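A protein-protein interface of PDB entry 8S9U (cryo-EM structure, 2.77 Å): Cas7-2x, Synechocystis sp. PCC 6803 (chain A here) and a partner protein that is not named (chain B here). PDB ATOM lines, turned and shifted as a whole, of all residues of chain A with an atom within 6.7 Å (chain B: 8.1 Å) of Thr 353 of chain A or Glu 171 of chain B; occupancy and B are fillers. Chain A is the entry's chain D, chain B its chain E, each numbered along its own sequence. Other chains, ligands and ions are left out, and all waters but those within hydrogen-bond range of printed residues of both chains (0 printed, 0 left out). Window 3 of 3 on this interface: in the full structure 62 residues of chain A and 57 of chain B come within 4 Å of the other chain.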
ATOM      1  N   ALA A 244     -28.389  -1.195  -8.057  1.00  0.00           N
ATOM      2  CA  ALA A 244     -27.067  -1.763  -8.284  1.00  0.00           C
ATOM      3  C   ALA A 244     -26.603  -2.610  -7.117  1.00  0.00           C
ATOM      4  O   ALA A 244     -25.890  -3.594  -7.322  1.00  0.00           O
ATOM      5  CB  ALA A 244     -26.059  -0.653  -8.541  1.00  0.00           C
ATOM      6  N   GLU A 351     -26.055   0.008 -12.215  1.00  0.00           N
ATOM      7  CA  GLU A 351     -25.111  -0.976 -12.719  1.00  0.00           C
ATOM      8  C   GLU A 351     -23.884  -0.954 -11.827  1.00  0.00           C
ATOM      9  O   GLU A 351     -23.270   0.100 -11.653  1.00  0.00           O
ATOM     10  CB  GLU A 351     -24.721  -0.684 -14.169  1.00  0.00           C
ATOM     11  CG  GLU A 351     -25.851  -0.797 -15.168  1.00  0.00           C
ATOM     12  CD  GLU A 351     -26.443  -2.191 -15.232  1.00  0.00           C
ATOM     13  OE1 GLU A 351     -25.694  -3.171 -15.026  1.00  0.00           O
ATOM     14  OE2 GLU A 351     -27.660  -2.309 -15.482  1.00  0.00           O
ATOM     15  N   MET A 352     -23.519  -2.112 -11.273  1.00  0.00           N
ATOM     16  CA  MET A 352     -22.451  -2.141 -10.282  1.00  0.00           C
ATOM     17  C   MET A 352     -21.131  -1.689 -10.872  1.00  0.00           C
ATOM     18  O   MET A 352     -20.378  -0.952 -10.229  1.00  0.00           O
ATOM     19  CB  MET A 352     -22.286  -3.545  -9.711  1.00  0.00           C
ATOM     20  CG  MET A 352     -21.141  -3.645  -8.724  1.00  0.00           C
ATOM     21  SD  MET A 352     -20.877  -5.264  -8.003  1.00  0.00           S
ATOM     22  CE  MET A 352     -22.313  -5.391  -6.974  1.00  0.00           C
ATOM     23  N   THR A 353     -20.833  -2.108 -12.087  1.00  0.00           N
ATOM     24  CA  THR A 353     -19.650  -1.634 -12.782  1.00  0.00           C
ATOM     25  C   THR A 353     -19.926  -0.416 -13.639  1.00  0.00           C
ATOM     26  O   THR A 353     -19.003   0.107 -14.266  1.00  0.00           O
ATOM     27  CB  THR A 353     -19.047  -2.747 -13.624  1.00  0.00           C
ATOM     28  OG1 THR A 353     -20.023  -3.229 -14.551  1.00  0.00           O
ATOM     29  CG2 THR A 353     -18.612  -3.874 -12.720  1.00  0.00           C
ATOM     30  N   GLY A 354     -21.176   0.022 -13.707  1.00  0.00           N
ATOM     31  CA  GLY A 354     -21.488   1.239 -14.414  1.00  0.00           C
ATOM     32  C   GLY A 354     -21.537   2.451 -13.518  1.00  0.00           C
ATOM     33  O   GLY A 354     -20.569   2.764 -12.825  1.00  0.00           O
ATOM     34  N   ASN A 355     -22.669   3.144 -13.535  1.00  0.00           N
ATOM     35  CA  ASN A 355     -22.815   4.403 -12.820  1.00  0.00           C
ATOM     36  C   ASN A 355     -22.599   4.295 -11.316  1.00  0.00           C
ATOM     37  O   ASN A 355     -22.427   5.328 -10.665  1.00  0.00           O
ATOM     38  CB  ASN A 355     -24.184   5.005 -13.131  1.00  0.00           C
ATOM     39  CG  ASN A 355     -25.309   4.048 -12.880  1.00  0.00           C
ATOM     40  OD1 ASN A 355     -25.161   3.084 -12.151  1.00  0.00           O
ATOM     41  ND2 ASN A 355     -26.452   4.315 -13.479  1.00  0.00           N
ATOM     42  N   LEU A 356     -22.616   3.091 -10.740  1.00  0.00           N
ATOM     43  CA  LEU A 356     -22.290   2.945  -9.322  1.00  0.00           C
ATOM     44  C   LEU A 356     -20.857   3.336  -9.015  1.00  0.00           C
ATOM     45  O   LEU A 356     -20.583   3.912  -7.962  1.00  0.00           O
ATOM     46  CB  LEU A 356     -22.529   1.516  -8.853  1.00  0.00           C
ATOM     47  CG  LEU A 356     -22.290   1.247  -7.366  1.00  0.00           C
ATOM     48  CD1 LEU A 356     -23.402   1.769  -6.516  1.00  0.00           C
ATOM     49  CD2 LEU A 356     -22.090  -0.224  -7.119  1.00  0.00           C
ATOM     50  N   GLN A 357     -19.927   3.015  -9.895  1.00  0.00           N
ATOM     51  CA  GLN A 357     -18.538   3.359  -9.613  1.00  0.00           C
ATOM     52  C   GLN A 357     -18.316   4.851  -9.424  1.00  0.00           C
ATOM     53  O   GLN A 357     -17.691   5.229  -8.421  1.00  0.00           O
ATOM     54  CB  GLN A 357     -17.626   2.780 -10.692  1.00  0.00           C
ATOM     55  CG  GLN A 357     -17.348   1.322 -10.499  1.00  0.00           C
ATOM     56  CD  GLN A 357     -16.468   0.762 -11.566  1.00  0.00           C
ATOM     57  OE1 GLN A 357     -16.015   1.484 -12.446  1.00  0.00           O
ATOM     58  NE2 GLN A 357     -16.187  -0.526 -11.484  1.00  0.00           N
ATOM     59  N   PRO A 358     -18.773   5.742 -10.312  1.00  0.00           N
ATOM     60  CA  PRO A 358     -18.718   7.171  -9.981  1.00  0.00           C
ATOM     61  C   PRO A 358     -19.436   7.536  -8.701  1.00  0.00           C
ATOM     62  O   PRO A 358     -18.929   8.358  -7.937  1.00  0.00           O
ATOM     63  CB  PRO A 358     -19.369   7.819 -11.199  1.00  0.00           C
ATOM     64  CG  PRO A 358     -19.078   6.914 -12.274  1.00  0.00           C
ATOM     65  CD  PRO A 358     -19.204   5.555 -11.704  1.00  0.00           C
ATOM     66  N   TYR A 374     -13.054   2.122  -2.851  1.00  0.00           N
ATOM     67  CA  TYR A 374     -13.492   0.793  -2.449  1.00  0.00           C
ATOM     68  C   TYR A 374     -12.748   0.234  -1.250  1.00  0.00           C
ATOM     69  O   TYR A 374     -13.081  -0.865  -0.806  1.00  0.00           O
ATOM     70  CB  TYR A 374     -13.376  -0.171  -3.622  1.00  0.00           C
ATOM     71  CG  TYR A 374     -14.439   0.015  -4.669  1.00  0.00           C
ATOM     72  CD1 TYR A 374     -15.346   1.049  -4.590  1.00  0.00           C
ATOM     73  CD2 TYR A 374     -14.561  -0.871  -5.712  1.00  0.00           C
ATOM     74  CE1 TYR A 374     -16.302   1.225  -5.543  1.00  0.00           C
ATOM     75  CE2 TYR A 374     -15.527  -0.716  -6.654  1.00  0.00           C
ATOM     76  CZ  TYR A 374     -16.393   0.335  -6.569  1.00  0.00           C
ATOM     77  OH  TYR A 374     -17.378   0.466  -7.504  1.00  0.00           O
ATOM     78  N   PRO B 166     -12.008 -13.161  -6.719  1.00  0.00           N
ATOM     79  CA  PRO B 166     -12.290 -12.127  -7.717  1.00  0.00           C
ATOM     80  C   PRO B 166     -13.176 -11.029  -7.148  1.00  0.00           C
ATOM     81  O   PRO B 166     -14.161 -11.300  -6.462  1.00  0.00           O
ATOM     82  CB  PRO B 166     -12.996 -12.901  -8.830  1.00  0.00           C
ATOM     83  CG  PRO B 166     -13.612 -14.027  -8.146  1.00  0.00           C
ATOM     84  CD  PRO B 166     -12.689 -14.422  -7.042  1.00  0.00           C
ATOM     85  N   ASP B 167     -12.809  -9.785  -7.425  1.00  0.00           N
ATOM     86  CA  ASP B 167     -13.598  -8.625  -7.027  1.00  0.00           C
ATOM     87  C   ASP B 167     -14.477  -8.254  -8.215  1.00  0.00           C
ATOM     88  O   ASP B 167     -14.037  -7.570  -9.136  1.00  0.00           O
ATOM     89  CB  ASP B 167     -12.702  -7.466  -6.618  1.00  0.00           C
ATOM     90  CG  ASP B 167     -13.442  -6.415  -5.837  1.00  0.00           C
ATOM     91  OD1 ASP B 167     -14.683  -6.466  -5.805  1.00  0.00           O
ATOM     92  OD2 ASP B 167     -12.784  -5.532  -5.254  1.00  0.00           O
ATOM     93  N   ALA B 168     -15.720  -8.729  -8.202  1.00  0.00           N
ATOM     94  CA  ALA B 168     -16.645  -8.420  -9.280  1.00  0.00           C
ATOM     95  C   ALA B 168     -17.072  -6.962  -9.305  1.00  0.00           C
ATOM     96  O   ALA B 168     -17.595  -6.507 -10.324  1.00  0.00           O
ATOM     97  CB  ALA B 168     -17.875  -9.310  -9.173  1.00  0.00           C
ATOM     98  N   SER B 169     -16.863  -6.222  -8.219  1.00  0.00           N
ATOM     99  CA  SER B 169     -17.112  -4.785  -8.241  1.00  0.00           C
ATOM    100  C   SER B 169     -16.141  -4.046  -9.147  1.00  0.00           C
ATOM    101  O   SER B 169     -16.467  -2.969  -9.651  1.00  0.00           O
ATOM    102  CB  SER B 169     -17.033  -4.222  -6.832  1.00  0.00           C
ATOM    103  OG  SER B 169     -15.687  -4.143  -6.411  1.00  0.00           O
ATOM    104  N   LYS B 170     -14.955  -4.601  -9.366  1.00  0.00           N
ATOM    105  CA  LYS B 170     -13.923  -3.962 -10.167  1.00  0.00           C
ATOM    106  C   LYS B 170     -13.618  -4.755 -11.429  1.00  0.00           C
ATOM    107  O   LYS B 170     -12.555  -4.579 -12.025  1.00  0.00           O
ATOM    108  CB  LYS B 170     -12.655  -3.779  -9.333  1.00  0.00           C
ATOM    109  CG  LYS B 170     -12.824  -2.780  -8.212  1.00  0.00           C
ATOM    110  CD  LYS B 170     -11.578  -2.599  -7.368  1.00  0.00           C
ATOM    111  CE  LYS B 170     -10.391  -2.190  -8.198  1.00  0.00           C
ATOM    112  NZ  LYS B 170      -9.167  -2.059  -7.364  1.00  0.00           N
ATOM    113  N   GLU B 171     -14.532  -5.624 -11.846  1.00  0.00           N
ATOM    114  CA  GLU B 171     -14.359  -6.366 -13.083  1.00  0.00           C
ATOM    115  C   GLU B 171     -14.363  -5.416 -14.267  1.00  0.00           C
ATOM    116  O   GLU B 171     -15.121  -4.446 -14.307  1.00  0.00           O
ATOM    117  CB  GLU B 171     -15.455  -7.412 -13.258  1.00  0.00           C
ATOM    118  CG  GLU B 171     -16.806  -6.825 -13.538  1.00  0.00           C
ATOM    119  CD  GLU B 171     -17.894  -7.854 -13.669  1.00  0.00           C
ATOM    120  OE1 GLU B 171     -17.815  -8.907 -13.013  1.00  0.00           O
ATOM    121  OE2 GLU B 171     -18.831  -7.609 -14.452  1.00  0.00           O
ATOM    122  N   GLU B 172     -13.474  -5.668 -15.211  1.00  0.00           N
ATOM    123  CA  GLU B 172     -13.338  -4.844 -16.394  1.00  0.00           C
ATOM    124  C   GLU B 172     -13.565  -5.712 -17.618  1.00  0.00           C
ATOM    125  O   GLU B 172     -13.176  -6.878 -17.634  1.00  0.00           O
ATOM    126  CB  GLU B 172     -11.951  -4.231 -16.424  1.00  0.00           C
ATOM    127  CG  GLU B 172     -11.793  -3.095 -15.445  1.00  0.00           C
ATOM    128  CD  GLU B 172     -10.426  -2.462 -15.501  1.00  0.00           C
ATOM    129  OE1 GLU B 172      -9.447  -3.198 -15.739  1.00  0.00           O
ATOM    130  OE2 GLU B 172     -10.323  -1.235 -15.290  1.00  0.00           O
ATOM    131  N   ILE B 173     -14.184  -5.145 -18.651  1.00  0.00           N
ATOM    132  CA  ILE B 173     -14.740  -5.937 -19.741  1.00  0.00           C
ATOM    133  C   ILE B 173     -14.175  -5.410 -21.048  1.00  0.00           C
ATOM    134  O   ILE B 173     -14.156  -4.197 -21.276  1.00  0.00           O
ATOM    135  CB  ILE B 173     -16.278  -5.882 -19.770  1.00  0.00           C
ATOM    136  CG1 ILE B 173     -16.860  -6.291 -18.433  1.00  0.00           C
ATOM    137  CG2 ILE B 173     -16.807  -6.848 -20.768  1.00  0.00           C
ATOM    138  CD1 ILE B 173     -17.259  -5.129 -17.577  1.00  0.00           C
ATOM    139  N   ASN B 174     -13.732  -6.321 -21.906  1.00  0.00           N
ATOM    140  CA  ASN B 174     -13.496  -6.057 -23.314  1.00  0.00           C
ATOM    141  C   ASN B 174     -14.127  -7.173 -24.118  1.00  0.00           C
ATOM    142  O   ASN B 174     -13.993  -8.346 -23.764  1.00  0.00           O
ATOM    143  CB  ASN B 174     -12.013  -5.996 -23.642  1.00  0.00           C
ATOM    144  CG  ASN B 174     -11.327  -4.824 -23.004  1.00  0.00           C
ATOM    145  OD1 ASN B 174     -10.872  -4.903 -21.865  1.00  0.00           O
ATOM    146  ND2 ASN B 174     -11.228  -3.725 -23.741  1.00  0.00           N
ATOM    147  N   HIS B 177     -15.576 -10.113 -22.599  1.00  0.00           N
ATOM    148  CA  HIS B 177     -14.722 -10.898 -21.715  1.00  0.00           C
ATOM    149  C   HIS B 177     -14.383 -10.112 -20.451  1.00  0.00           C
ATOM    150  O   HIS B 177     -13.956  -8.962 -20.528  1.00  0.00           O
ATOM    151  CB  HIS B 177     -13.461 -11.299 -22.471  1.00  0.00           C
ATOM    152  CG  HIS B 177     -12.400 -11.929 -21.629  1.00  0.00           C
ATOM    153  ND1 HIS B 177     -12.362 -13.280 -21.378  1.00  0.00           N
ATOM    154  CD2 HIS B 177     -11.286 -11.414 -21.065  1.00  0.00           C
ATOM    155  CE1 HIS B 177     -11.299 -13.564 -20.653  1.00  0.00           C
ATOM    156  NE2 HIS B 177     -10.629 -12.448 -20.450  1.00  0.00           N
ATOM    157  N   LYS B 178     -14.552 -10.743 -19.292  1.00  0.00           N
ATOM    158  CA  LYS B 178     -14.375 -10.098 -17.994  1.00  0.00           C
ATOM    159  C   LYS B 178     -13.029 -10.434 -17.370  1.00  0.00           C
ATOM    160  O   LYS B 178     -12.645 -11.603 -17.303  1.00  0.00           O
ATOM    161  CB  LYS B 178     -15.484 -10.496 -17.029  1.00  0.00           C
ATOM    162  CG  LYS B 178     -16.855 -10.086 -17.442  1.00  0.00           C
ATOM    163  CD  LYS B 178     -17.853 -10.549 -16.409  1.00  0.00           C
ATOM    164  CE  LYS B 178     -19.254 -10.167 -16.785  1.00  0.00           C
ATOM    165  NZ  LYS B 178     -19.422  -8.699 -16.679  1.00  0.00           N
ATOM    166  N   THR B 179     -12.323  -9.407 -16.912  1.00  0.00           N
ATOM    167  CA  THR B 179     -11.074  -9.550 -16.179  1.00  0.00           C
ATOM    168  C   THR B 179     -11.274  -9.110 -14.737  1.00  0.00           C
ATOM    169  O   THR B 179     -11.761  -8.006 -14.488  1.00  0.00           O
ATOM    170  CB  THR B 179      -9.971  -8.719 -16.822  1.00  0.00           C
ATOM    171  OG1 THR B 179      -9.904  -9.020 -18.217  1.00  0.00           O
ATOM    172  CG2 THR B 179      -8.649  -9.030 -16.196  1.00  0.00           C
ATOM    173  N   TYR B 180     -10.932  -9.982 -13.795  1.00  0.00           N
ATOM    174  CA  TYR B 180     -11.142  -9.744 -12.376  1.00  0.00           C
ATOM    175  C   TYR B 180      -9.827  -9.457 -11.674  1.00  0.00           C
ATOM    176  O   TYR B 180      -8.875 -10.232 -11.823  1.00  0.00           O
ATOM    177  CB  TYR B 180     -11.806 -10.951 -11.732  1.00  0.00           C
ATOM    178  CG  TYR B 180     -13.207 -11.196 -12.199  1.00  0.00           C
ATOM    179  CD1 TYR B 180     -13.458 -11.976 -13.306  1.00  0.00           C
ATOM    180  CD2 TYR B 180     -14.278 -10.651 -11.532  1.00  0.00           C
ATOM    181  CE1 TYR B 180     -14.731 -12.217 -13.720  1.00  0.00           C
ATOM    182  CE2 TYR B 180     -15.552 -10.876 -11.950  1.00  0.00           C
ATOM    183  CZ  TYR B 180     -15.774 -11.663 -13.041  1.00  0.00           C
ATOM    184  OH  TYR B 180     -17.055 -11.872 -13.477  1.00  0.00           O
ATOM    185  N   PRO B 181      -9.725  -8.381 -10.906  1.00  0.00           N
ATOM    186  CA  PRO B 181      -8.656  -8.269  -9.915  1.00  0.00           C
ATOM    187  C   PRO B 181      -8.951  -9.123  -8.690  1.00  0.00           C
ATOM    188  O   PRO B 181     -10.050  -9.641  -8.509  1.00  0.00           O
ATOM    189  CB  PRO B 181      -8.660  -6.784  -9.579  1.00  0.00           C
ATOM    190  CG  PRO B 181     -10.058  -6.386  -9.763  1.00  0.00           C
ATOM    191  CD  PRO B 181     -10.644  -7.236 -10.843  1.00  0.00           C
ATOM    192  N   ARG B 619     -13.340 -16.268 -18.099  1.00  0.00           N
ATOM    193  CA  ARG B 619     -12.906 -15.055 -17.427  1.00  0.00           C
ATOM    194  C   ARG B 619     -11.392 -14.965 -17.435  1.00  0.00           C
ATOM    195  O   ARG B 619     -10.684 -15.912 -17.766  1.00  0.00           O
ATOM    196  CB  ARG B 619     -13.407 -15.005 -15.985  1.00  0.00           C
ATOM    197  CG  ARG B 619     -12.823 -16.086 -15.126  1.00  0.00           C
ATOM    198  CD  ARG B 619     -13.271 -15.971 -13.705  1.00  0.00           C
ATOM    199  NE  ARG B 619     -14.712 -16.124 -13.580  1.00  0.00           N
ATOM    200  CZ  ARG B 619     -15.395 -15.793 -12.496  1.00  0.00           C
ATOM    201  NH1 ARG B 619     -14.759 -15.336 -11.436  1.00  0.00           N
ATOM    202  NH2 ARG B 619     -16.704 -15.954 -12.458  1.00  0.00           N
ATOM    203  N   SER B 620     -10.899 -13.816 -17.017  1.00  0.00           N
ATOM    204  CA  SER B 620      -9.486 -13.628 -16.770  1.00  0.00           C
ATOM    205  C   SER B 620      -9.309 -13.027 -15.388  1.00  0.00           C
ATOM    206  O   SER B 620     -10.200 -12.352 -14.877  1.00  0.00           O
ATOM    207  CB  SER B 620      -8.884 -12.732 -17.833  1.00  0.00           C
ATOM    208  OG  SER B 620      -7.510 -12.553 -17.624  1.00  0.00           O
ATOM    209  N   LYS B 622      -6.526 -10.818 -12.874  1.00  0.00           N
ATOM    210  CA  LYS B 622      -5.349  -9.960 -12.867  1.00  0.00           C
ATOM    211  C   LYS B 622      -4.274 -10.446 -11.915  1.00  0.00           C
ATOM    212  O   LYS B 622      -3.179  -9.876 -11.903  1.00  0.00           O
ATOM    213  CB  LYS B 622      -5.727  -8.529 -12.501  1.00  0.00           C
ATOM    214  CG  LYS B 622      -6.762  -7.931 -13.400  1.00  0.00           C
ATOM    215  CD  LYS B 622      -6.869  -6.443 -13.210  1.00  0.00           C
ATOM    216  CE  LYS B 622      -7.895  -5.862 -14.163  1.00  0.00           C
ATOM    217  NZ  LYS B 622      -7.947  -4.381 -14.087  1.00  0.00           N
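The backbone carbonyl oxygen of Ser 169 of chain B lies within hydrogen-bond range of the side-chain amide nitrogen of Gln 357 of chain A (3.1 Å).
OH of Tyr 180 of chain B is in hydrogen-bond range of OE1 of Glu 171 of chain B (3.1 Å).
The side-chain carboxylate (OE2) of Glu 171 of chain B is in salt-bridge range of the side-chain amino group (NZ) of Lys 178 of chain B, 2.5 Å away.
OG of Ser 169 of chain B lies within hydrogen-bond range of OD1 of Asp 167 of chain B, 2.6 Å away.
Among the printed residues, pairs that only touch across the chains: Met 352 of chain A with Ser 169 of chain B (3.8 Å), Thr 353 of chain A with Ala 168 of chain B (3.7 Å), Thr 353 of chain A with Ser 169 of chain B (3.9 Å), Thr 353 of chain A with Glu 171 of chain B (3.6 Å), Tyr 374 of chain A with Ser 169 of chain B (3.4 Å) and Tyr 374 of chain A with Lys 170 of chain B (3.6 Å).
Of chain B, only Ala 168 (3.7 Å), Ser 169 (3.9 Å) and Glu 171 (3.6 Å) come within 4 Å of Thr 353 of chain A.
Glu 171 of chain B touches one residue of chain A.
Printed residues of chain A within 4 Å of Lys 170 of chain B: Tyr 374.
Printed residues of chain A within 4 Å of Ala 168 of chain B: Thr 353.
Arg 619 of chain B touches none of the printed residues of chain A.
The nearest residue of chain B that does not touch Thr 353 of chain A is Ile 173 of chain B (4.5 Å).
Of the 17 printed residues of chain B, 4 touch a printed residue of chain A.
Of the 10 printed residues of chain A, 4 touch a printed residue of chain B.
Printed residues of chain A that touch a printed residue of chain B: Met 352, Thr 353, Gln 357 and Tyr 374.
Among the printed residues, 7 pairs touch across the chains.
Among the printed residues, no Asp or Glu carboxylate lies within 4 Å of a Lys or Arg side-chain nitrogen of the other chain.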
